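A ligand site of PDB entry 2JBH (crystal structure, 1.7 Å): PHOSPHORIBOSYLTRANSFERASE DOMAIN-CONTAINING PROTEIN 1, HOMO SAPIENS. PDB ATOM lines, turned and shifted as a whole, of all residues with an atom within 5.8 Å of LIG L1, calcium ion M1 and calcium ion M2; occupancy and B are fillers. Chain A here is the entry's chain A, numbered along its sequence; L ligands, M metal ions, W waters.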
ATOM      1  N   VAL A  74      19.070  -2.599  23.484  1.00  0.00           N
ATOM      2  CA  VAL A  74      19.284  -2.723  22.042  1.00  0.00           C
ATOM      3  C   VAL A  74      19.967  -1.440  21.507  1.00  0.00           C
ATOM      4  O   VAL A  74      19.304  -0.419  21.289  1.00  0.00           O
ATOM      5  CB  VAL A  74      17.964  -2.974  21.264  1.00  0.00           C
ATOM      6  CG1 VAL A  74      18.286  -3.309  19.811  1.00  0.00           C
ATOM      7  CG2 VAL A  74      17.165  -4.135  21.928  1.00  0.00           C
ATOM      8  N   LEU A  75      21.284  -1.512  21.403  1.00  0.00           N
ATOM      9  CA  LEU A  75      22.120  -0.405  20.912  1.00  0.00           C
ATOM     10  C   LEU A  75      21.888  -0.181  19.387  1.00  0.00           C
ATOM     11  O   LEU A  75      21.480  -1.102  18.700  1.00  0.00           O
ATOM     12  CB  LEU A  75      23.599  -0.730  21.143  1.00  0.00           C
ATOM     13  CG  LEU A  75      24.077  -0.798  22.585  1.00  0.00           C
ATOM     14  CD1 LEU A  75      25.525  -1.316  22.600  1.00  0.00           C
ATOM     15  CD2 LEU A  75      23.948   0.534  23.247  1.00  0.00           C
ATOM     16  N   GLY A  77      20.277   2.950  19.394  1.00  0.00           N
ATOM     17  CA  GLY A  77      19.109   3.804  19.628  1.00  0.00           C
ATOM     18  C   GLY A  77      18.446   3.616  20.986  1.00  0.00           C
ATOM     19  O   GLY A  77      17.819   4.525  21.476  1.00  0.00           O
ATOM     20  N   GLY A  78      18.584   2.424  21.577  1.00  0.00           N
ATOM     21  CA  GLY A  78      17.966   2.172  22.881  1.00  0.00           C
ATOM     22  C   GLY A  78      18.708   2.760  24.072  1.00  0.00           C
ATOM     23  O   GLY A  78      18.177   2.707  25.209  1.00  0.00           O
ATOM     24  N   GLU A 141      14.195  -1.178  23.859  1.00  0.00           N
ATOM     25  CA  GLU A 141      14.305  -0.830  22.433  1.00  0.00           C
ATOM     26  C   GLU A 141      13.820   0.603  22.196  1.00  0.00           C
ATOM     27  O   GLU A 141      13.015   1.125  22.971  1.00  0.00           O
ATOM     28  CB  GLU A 141      13.448  -1.841  21.628  1.00  0.00           C
ATOM     29  CG  GLU A 141      13.185  -1.505  20.126  1.00  0.00           C
ATOM     30  CD  GLU A 141      14.433  -1.492  19.234  1.00  0.00           C
ATOM     31  OE1 GLU A 141      14.314  -1.828  18.011  1.00  0.00           O
ATOM     32  OE2 GLU A 141      15.545  -1.135  19.716  1.00  0.00           O
ATOM     33  N   ASP A 142      14.289   1.226  21.125  1.00  0.00           N
ATOM     34  CA  ASP A 142      13.903   2.623  20.839  1.00  0.00           C
ATOM     35  C   ASP A 142      12.521   2.795  20.226  1.00  0.00           C
ATOM     36  O   ASP A 142      11.675   3.529  20.756  1.00  0.00           O
ATOM     37  CB  ASP A 142      14.976   3.387  20.026  1.00  0.00           C
ATOM     38  CG  ASP A 142      15.431   2.673  18.740  1.00  0.00           C
ATOM     39  OD1 ASP A 142      15.090   1.487  18.491  1.00  0.00           O
ATOM     40  OD2 ASP A 142      16.193   3.320  17.972  1.00  0.00           O
ATOM     41  N   VAL A 143      12.284   2.122  19.107  1.00  0.00           N
ATOM     42  CA  VAL A 143      11.047   2.332  18.352  1.00  0.00           C
ATOM     43  C   VAL A 143      10.675   1.081  17.554  1.00  0.00           C
ATOM     44  O   VAL A 143      11.524   0.432  16.931  1.00  0.00           O
ATOM     45  CB  VAL A 143      11.130   3.625  17.435  1.00  0.00           C
ATOM     46  CG1 VAL A 143      12.380   3.585  16.567  1.00  0.00           C
ATOM     47  CG2 VAL A 143       9.866   3.814  16.575  1.00  0.00           C
ATOM     48  N   VAL A 144       9.386   0.757  17.609  1.00  0.00           N
ATOM     49  CA  VAL A 144       8.817  -0.313  16.813  1.00  0.00           C
ATOM     50  C   VAL A 144       8.133   0.328  15.604  1.00  0.00           C
ATOM     51  O   VAL A 144       7.277   1.195  15.752  1.00  0.00           O
ATOM     52  CB  VAL A 144       7.758  -1.075  17.660  1.00  0.00           C
ATOM     53  CG1 VAL A 144       7.024  -2.069  16.798  1.00  0.00           C
ATOM     54  CG2 VAL A 144       8.435  -1.795  18.805  1.00  0.00           C
ATOM     55  N   GLY A 145       8.555  -0.102  14.417  1.00  0.00           N
ATOM     56  CA  GLY A 145       7.926   0.364  13.162  1.00  0.00           C
ATOM     57  C   GLY A 145       6.997  -0.726  12.649  1.00  0.00           C
ATOM     58  O   GLY A 145       5.821  -0.742  12.999  1.00  0.00           O
ATOM     59  N   THR A 146       7.519  -1.638  11.848  1.00  0.00           N
ATOM     60  CA  THR A 146       6.743  -2.798  11.354  1.00  0.00           C
ATOM     61  C   THR A 146       6.580  -3.889  12.423  1.00  0.00           C
ATOM     62  O   THR A 146       5.679  -4.746  12.350  1.00  0.00           O
ATOM     63  CB  THR A 146       7.369  -3.422  10.082  1.00  0.00           C
ATOM     64  OG1 THR A 146       8.631  -4.024  10.410  1.00  0.00           O
ATOM     65  CG2 THR A 146       7.563  -2.364   9.010  1.00  0.00           C
ATOM     66  N   GLY A 147       7.480  -3.867  13.405  1.00  0.00           N
ATOM     67  CA  GLY A 147       7.546  -4.918  14.420  1.00  0.00           C
ATOM     68  C   GLY A 147       8.386  -6.122  14.025  1.00  0.00           C
ATOM     69  O   GLY A 147       8.602  -7.023  14.848  1.00  0.00           O
ATOM     70  N   ARG A 148       8.889  -6.144  12.785  1.00  0.00           N
ATOM     71  CA  ARG A 148       9.725  -7.263  12.329  1.00  0.00           C
ATOM     72  C   ARG A 148      10.977  -7.495  13.174  1.00  0.00           C
ATOM     73  O   ARG A 148      11.345  -8.647  13.489  1.00  0.00           O
ATOM     74  CB  ARG A 148      10.081  -7.091  10.850  1.00  0.00           C
ATOM     75  CG  ARG A 148       8.891  -7.322   9.914  1.00  0.00           C
ATOM     76  CD  ARG A 148       9.319  -7.186   8.449  1.00  0.00           C
ATOM     77  NE  ARG A 148       9.711  -5.804   8.129  1.00  0.00           N
ATOM     78  CZ  ARG A 148      10.108  -5.383   6.929  1.00  0.00           C
ATOM     79  NH1 ARG A 148      10.174  -6.231   5.907  1.00  0.00           N
ATOM     80  NH2 ARG A 148      10.452  -4.117   6.755  1.00  0.00           N
ATOM     81  N   THR A 149      11.638  -6.403  13.573  1.00  0.00           N
ATOM     82  CA  THR A 149      12.872  -6.506  14.356  1.00  0.00           C
ATOM     83  C   THR A 149      12.619  -7.156  15.712  1.00  0.00           C
ATOM     84  O   THR A 149      13.333  -8.080  16.114  1.00  0.00           O
ATOM     85  CB  THR A 149      13.498  -5.117  14.506  1.00  0.00           C
ATOM     86  OG1 THR A 149      13.810  -4.623  13.207  1.00  0.00           O
ATOM     87  CG2 THR A 149      14.780  -5.147  15.363  1.00  0.00           C
ATOM     88  N   MET A 150      11.603  -6.677  16.412  1.00  0.00           N
ATOM     89  CA  MET A 150      11.280  -7.226  17.724  1.00  0.00           C
ATOM     90  C   MET A 150      10.811  -8.678  17.645  1.00  0.00           C
ATOM     91  O   MET A 150      11.167  -9.489  18.501  1.00  0.00           O
ATOM     92  CB  MET A 150      10.275  -6.358  18.459  1.00  0.00           C
ATOM     93  CG  MET A 150      10.883  -5.031  19.011  1.00  0.00           C
ATOM     94  SD  MET A 150      12.225  -5.320  20.202  1.00  0.00           S
ATOM     95  CE  MET A 150      13.670  -5.088  19.159  1.00  0.00           C
ATOM     96  N   LYS A 173       4.986   2.924  16.370  1.00  0.00           N
ATOM     97  CA  LYS A 173       4.271   3.649  15.307  1.00  0.00           C
ATOM     98  C   LYS A 173       2.899   3.040  15.049  1.00  0.00           C
ATOM     99  O   LYS A 173       2.744   1.815  15.075  1.00  0.00           O
ATOM    100  CB  LYS A 173       5.088   3.645  14.013  1.00  0.00           C
ATOM    101  CG  LYS A 173       6.452   4.321  14.184  1.00  0.00           C
ATOM    102  CD  LYS A 173       7.251   4.454  12.869  1.00  0.00           C
ATOM    103  CE  LYS A 173       8.637   5.011  13.163  1.00  0.00           C
ATOM    104  NZ  LYS A 173       9.392   5.147  11.885  1.00  0.00           N
ATOM    105  N   LEU A 193       5.736   8.138  11.035  1.00  0.00           N
ATOM    106  CA  LEU A 193       6.701   9.031  10.426  1.00  0.00           C
ATOM    107  C   LEU A 193       8.075   8.709  10.995  1.00  0.00           C
ATOM    108  O   LEU A 193       8.190   7.797  11.810  1.00  0.00           O
ATOM    109  CB  LEU A 193       6.302  10.496  10.650  1.00  0.00           C
ATOM    110  CG  LEU A 193       5.830  10.904  12.039  1.00  0.00           C
ATOM    111  CD1 LEU A 193       6.983  10.875  12.989  1.00  0.00           C
ATOM    112  CD2 LEU A 193       5.181  12.282  12.060  1.00  0.00           C
ATOM    113  N   PHE A 194       9.100   9.427  10.529  1.00  0.00           N
ATOM    114  CA  PHE A 194      10.473   9.114  10.895  1.00  0.00           C
ATOM    115  C   PHE A 194      10.893  10.064  12.012  1.00  0.00           C
ATOM    116  O   PHE A 194      10.665  11.275  11.920  1.00  0.00           O
ATOM    117  CB  PHE A 194      11.384   9.301   9.680  1.00  0.00           C
ATOM    118  CG  PHE A 194      12.835   9.196  10.007  1.00  0.00           C
ATOM    119  CD1 PHE A 194      13.405   7.974  10.347  1.00  0.00           C
ATOM    120  CD2 PHE A 194      13.662  10.325   9.936  1.00  0.00           C
ATOM    121  CE1 PHE A 194      14.785   7.863  10.656  1.00  0.00           C
ATOM    122  CE2 PHE A 194      15.017  10.247  10.215  1.00  0.00           C
ATOM    123  CZ  PHE A 194      15.591   9.010  10.596  1.00  0.00           C
ATOM    124  N   VAL A 195      11.513   9.503  13.055  1.00  0.00           N
ATOM    125  CA  VAL A 195      11.891  10.308  14.233  1.00  0.00           C
ATOM    126  C   VAL A 195      13.363  10.157  14.594  1.00  0.00           C
ATOM    127  O   VAL A 195      13.962   9.107  14.352  1.00  0.00           O
ATOM    128  CB  VAL A 195      11.035   9.968  15.490  1.00  0.00           C
ATOM    129  CG1 VAL A 195       9.603  10.515  15.309  1.00  0.00           C
ATOM    130  CG2 VAL A 195      11.004   8.467  15.735  1.00  0.00           C
ATOM    131  N   VAL A 196      13.906  11.219  15.190  1.00  0.00           N
ATOM    132  CA  VAL A 196      15.296  11.248  15.669  1.00  0.00           C
ATOM    133  C   VAL A 196      15.304  11.914  17.049  1.00  0.00           C
ATOM    134  O   VAL A 196      14.301  12.530  17.468  1.00  0.00           O
ATOM    135  CB  VAL A 196      16.211  12.058  14.704  1.00  0.00           C
ATOM    136  CG1 VAL A 196      16.164  11.428  13.291  1.00  0.00           C
ATOM    137  CG2 VAL A 196      15.806  13.527  14.671  1.00  0.00           C
ATOM    138  N   LEU A 200      18.049   8.364  19.149  1.00  0.00           N
ATOM    139  CA  LEU A 200      17.625   7.864  17.827  1.00  0.00           C
ATOM    140  C   LEU A 200      18.284   8.711  16.746  1.00  0.00           C
ATOM    141  O   LEU A 200      18.350   9.931  16.899  1.00  0.00           O
ATOM    142  CB  LEU A 200      16.117   7.947  17.658  1.00  0.00           C
ATOM    143  CG  LEU A 200      15.245   6.917  18.386  1.00  0.00           C
ATOM    144  CD1 LEU A 200      15.276   7.077  19.943  1.00  0.00           C
ATOM    145  CD2 LEU A 200      13.810   7.017  17.909  1.00  0.00           C
ATOM    146  N   ASP A 201      18.737   8.069  15.669  1.00  0.00           N
ATOM    147  CA  ASP A 201      19.594   8.756  14.675  1.00  0.00           C
ATOM    148  C   ASP A 201      18.997   8.848  13.262  1.00  0.00           C
ATOM    149  O   ASP A 201      18.067   8.114  12.886  1.00  0.00           O
ATOM    150  CB  ASP A 201      20.953   8.078  14.541  1.00  0.00           C
ATOM    151  CG  ASP A 201      20.877   6.802  13.705  1.00  0.00           C
ATOM    152  OD1 ASP A 201      20.063   5.926  14.050  1.00  0.00           O
ATOM    153  OD2 ASP A 201      21.617   6.688  12.704  1.00  0.00           O
ATOM    154  N   TYR A 202      19.595   9.757  12.497  1.00  0.00           N
ATOM    155  CA  TYR A 202      19.540   9.752  11.033  1.00  0.00           C
ATOM    156  C   TYR A 202      20.990   9.763  10.588  1.00  0.00           C
ATOM    157  O   TYR A 202      21.715  10.734  10.830  1.00  0.00           O
ATOM    158  CB  TYR A 202      18.825  11.001  10.562  1.00  0.00           C
ATOM    159  CG  TYR A 202      18.818  11.195   9.058  1.00  0.00           C
ATOM    160  CD1 TYR A 202      18.250  10.229   8.227  1.00  0.00           C
ATOM    161  CD2 TYR A 202      19.322  12.354   8.478  1.00  0.00           C
ATOM    162  CE1 TYR A 202      18.226  10.382   6.839  1.00  0.00           C
ATOM    163  CE2 TYR A 202      19.296  12.543   7.062  1.00  0.00           C
ATOM    164  CZ  TYR A 202      18.745  11.559   6.275  1.00  0.00           C
ATOM    165  OH  TYR A 202      18.691  11.707   4.896  1.00  0.00           O
ATOM    166  N   ARG A 207      21.704  11.801  17.620  1.00  0.00           N
ATOM    167  CA  ARG A 207      21.637  11.015  18.851  1.00  0.00           C
ATOM    168  C   ARG A 207      21.790  11.909  20.092  1.00  0.00           C
ATOM    169  O   ARG A 207      21.325  11.547  21.167  1.00  0.00           O
ATOM    170  CB  ARG A 207      22.690   9.918  18.889  1.00  0.00           C
ATOM    171  CG  ARG A 207      22.602   8.956  17.710  1.00  0.00           C
ATOM    172  CD  ARG A 207      23.289   7.648  18.061  1.00  0.00           C
ATOM    173  NE  ARG A 207      23.462   6.784  16.894  1.00  0.00           N
ATOM    174  CZ  ARG A 207      22.590   5.839  16.499  1.00  0.00           C
ATOM    175  NH1 ARG A 207      21.429   5.694  17.109  1.00  0.00           N
ATOM    176  NH2 ARG A 207      22.874   5.071  15.436  1.00  0.00           N
HETATM  177  P1  LIG L   1      10.917  -2.485  12.434  1.00  0.00           P
HETATM  178  O1  LIG L   1       9.899  -2.342  13.606  1.00  0.00           O
HETATM  179  O2  LIG L   1      10.218  -1.989  11.079  1.00  0.00           O
HETATM  180  O3  LIG L   1      11.436  -3.866  12.254  1.00  0.00           O
HETATM  181  O4  LIG L   1      12.118  -1.446  12.719  1.00  0.00           O
HETATM  182  C1  LIG L   1      13.342  -1.562  11.992  1.00  0.00           C
HETATM  183  C2  LIG L   1      14.515  -0.887  12.780  1.00  0.00           C
HETATM  184  O5  LIG L   1      14.425   0.531  12.491  1.00  0.00           O
HETATM  185  C3  LIG L   1      14.434  -1.031  14.294  1.00  0.00           C
HETATM  186  O6  LIG L   1      15.774  -1.050  14.799  1.00  0.00           O
HETATM  187  C4  LIG L   1      13.708   0.258  14.698  1.00  0.00           C
HETATM  188  O7  LIG L   1      14.055   0.624  16.048  1.00  0.00           O
HETATM  189  C5  LIG L   1      14.327   1.274  13.734  1.00  0.00           C
HETATM  190  N1  LIG L   1      13.416   2.408  13.455  1.00  0.00           N
HETATM  191  C6  LIG L   1      12.159   2.303  12.983  1.00  0.00           C
HETATM  192  N2  LIG L   1      11.648   3.532  12.824  1.00  0.00           N
HETATM  193  C7  LIG L   1      12.586   4.415  13.167  1.00  0.00           C
HETATM  194  C8  LIG L   1      12.631   5.811  13.204  1.00  0.00           C
HETATM  195  O8  LIG L   1      11.685   6.539  12.894  1.00  0.00           O
HETATM  196  N3  LIG L   1      13.803   6.419  13.624  1.00  0.00           N
HETATM  197  C9  LIG L   1      14.897   5.663  14.011  1.00  0.00           C
HETATM  198  N4  LIG L   1      15.983   6.308  14.414  1.00  0.00           N
HETATM  199  N5  LIG L   1      14.858   4.329  13.957  1.00  0.00           N
HETATM  200  C10 LIG L   1      13.730   3.695  13.555  1.00  0.00           C
HETATM  201  P1  LG2 L   2      20.494   2.047  15.785  1.00  0.00           P
HETATM  202  O1  LG2 L   2      19.666   1.607  16.971  1.00  0.00           O
HETATM  203  O2  LG2 L   2      21.934   1.742  16.079  1.00  0.00           O
HETATM  204  O3  LG2 L   2      20.026   1.371  14.471  1.00  0.00           O
HETATM  205  O4  LG2 L   2      20.247   3.509  15.511  1.00  0.00           O
HETATM  206 CA    CA M   1      16.073  -0.336  17.268  1.00  0.00          CA
HETATM  207 CA    CA M   2      19.620   3.780  13.161  1.00  0.00          CA
HETATM  208  O   HOH W   1      17.420   2.926  13.878  1.00  0.00           O
HETATM  209  O   HOH W   2      12.763  -4.826   9.823  1.00  0.00           O
HETATM  210  O   HOH W   3      11.342  -2.343   8.645  1.00  0.00           O
HETATM  211  O   HOH W   4      17.689  -2.105  16.667  1.00  0.00           O
HETATM  212  O   HOH W   5      22.106   3.337  12.870  1.00  0.00           O
HETATM  213  O   HOH W   6      10.311  -4.136  15.689  1.00  0.00           O
HETATM  214  O   HOH W   7      17.906   4.961  16.304  1.00  0.00           O
HETATM  215  O   HOH W   8      17.416  -2.843  13.803  1.00  0.00           O
HETATM  216  O   HOH W   9      20.827   4.772  11.113  1.00  0.00           O
HETATM  217  O   HOH W  10      17.124   1.565  16.225  1.00  0.00           O
HETATM  218  O   HOH W  11      18.031   0.146  18.644  1.00  0.00           O
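Of the 23 residues printed, 1 comes within 4 Å of calcium ion M2. The nearest printed residue that does not touch calcium ion M2 is Arg 207 (4.2 Å).
Two residues have an atom within 4 Å of calcium ion M1: Glu 141 and Asp 142.
Val 144 touches LIG L1. Leu 193 touches LIG L1. Phe 194 touches LIG L1. CB of Leu 200 touches N4 of LIG L1 (3.6 Å). Hydrophobic or aromatic side chains within 4 Å of LIG L1: Val 143, Phe 194, Val 195 and Leu 200. 15 residues have an atom within 4 Å of LIG L1: Glu 141, Asp 142, Val 143, Val 144, Gly 145, Thr 146, Gly 147, Arg 148, Thr 149, Lys 173, Leu 193, Phe 194, Val 195, Leu 200 and Asp 201.
Calcium ion M1 is bound by the side-chain carboxylate (OD1) of Asp 142 (2.4 Å), water W10 (2.4 Å), the side-chain carboxylate (OE1) of Glu 141 (2.4 Å), water W11 (2.4 Å), water W4 (2.5 Å), an oxygen (O7) of LIG L1 (2.5 Å), an oxygen (O6) of LIG L1 (2.6 Å) and the side-chain carboxylate (OE2) of Glu 141 (2.6 Å). Calcium ion M1 has eight donor atoms within binding distance.
Water W5 bridges the guanidinium group of Arg 207 and the side-chain carboxylate of Asp 201. Water W3 lies within hydrogen-bond range of O2 of LIG L1 (2.7 Å) and NH2 of Arg 148 (2.7 Å). Water W6 lies within hydrogen-bond range of O1 of LIG L1 (2.8 Å), N of Met 150 (2.9 Å), N of Thr 149 (3.4 Å) and O of Gly 147 (3.5 Å). Water W7 lies within hydrogen-bond range of OD2 of Asp 142 (2.9 Å), N4 of LIG L1 (3.0 Å) and N of Asp 201 (3.3 Å).
The side-chain amino group of Lys 173 lies within hydrogen-bond range of the backbone carbonyl oxygen of Leu 193 (2.9 Å). The backbone NH (N) of Lys 173 sits at hydrogen-bond distance from the backbone carbonyl oxygen (O) of Val 144 (2.9 Å). The guanidinium group (NH2) of Arg 207 lies within salt-bridge range of the side-chain carboxylate (OD2) of Asp 201. The side-chain hydroxyl of Thr 146 is in hydrogen-bond range of the guanidinium group of Arg 148, at 3.1 Å.
An oxygen (O1) of LIG L1 sits at hydrogen-bond distance from the backbone NH (N) of Gly 147. A nitrogen (N3) of LIG L1 lies within hydrogen-bond range of the backbone carbonyl oxygen (O) of Val 195 (2.8 Å). The backbone NH (N) of Arg 148 is in hydrogen-bond range of an oxygen (O3) of LIG L1 (3.5 Å). N of Gly 145 sits at hydrogen-bond distance from O1 of LIG L1 (2.7 Å). O3 of LIG L1 sits at hydrogen-bond distance from OG1 of Thr 149 (2.7 Å). The backbone NH (N) of Thr 146 lies within hydrogen-bond range of an oxygen (O2) of LIG L1, at 2.8 Å. O of Asp 201 sits at hydrogen-bond distance from N4 of LIG L1, at 3.2 Å. The backbone NH (N) of Val 195 lies within hydrogen-bond range of an oxygen (O8) of LIG L1, 3.0 Å away. O2 of LIG L1 lies within hydrogen-bond range of OG1 of Thr 146 (2.7 Å). N of Thr 149 lies within hydrogen-bond range of O3 of LIG L1, 2.9 Å away. An oxygen (O8) of LIG L1 is in hydrogen-bond range of the side-chain amino group (NZ) of Lys 173 (2.9 Å). The backbone carbonyl oxygen of Val 143 sits close to an oxygen (O7) of LIG L1, at 2.7 Å.
Calcium ion M2 is bound by OD1 of Asp 201 (2.4 Å), O4 of LG2 L2 (2.4 Å), water W1 (2.5 Å), water W5 (2.5 Å), water W9 (2.6 Å) and O3 of LG2 L2 (2.8 Å).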
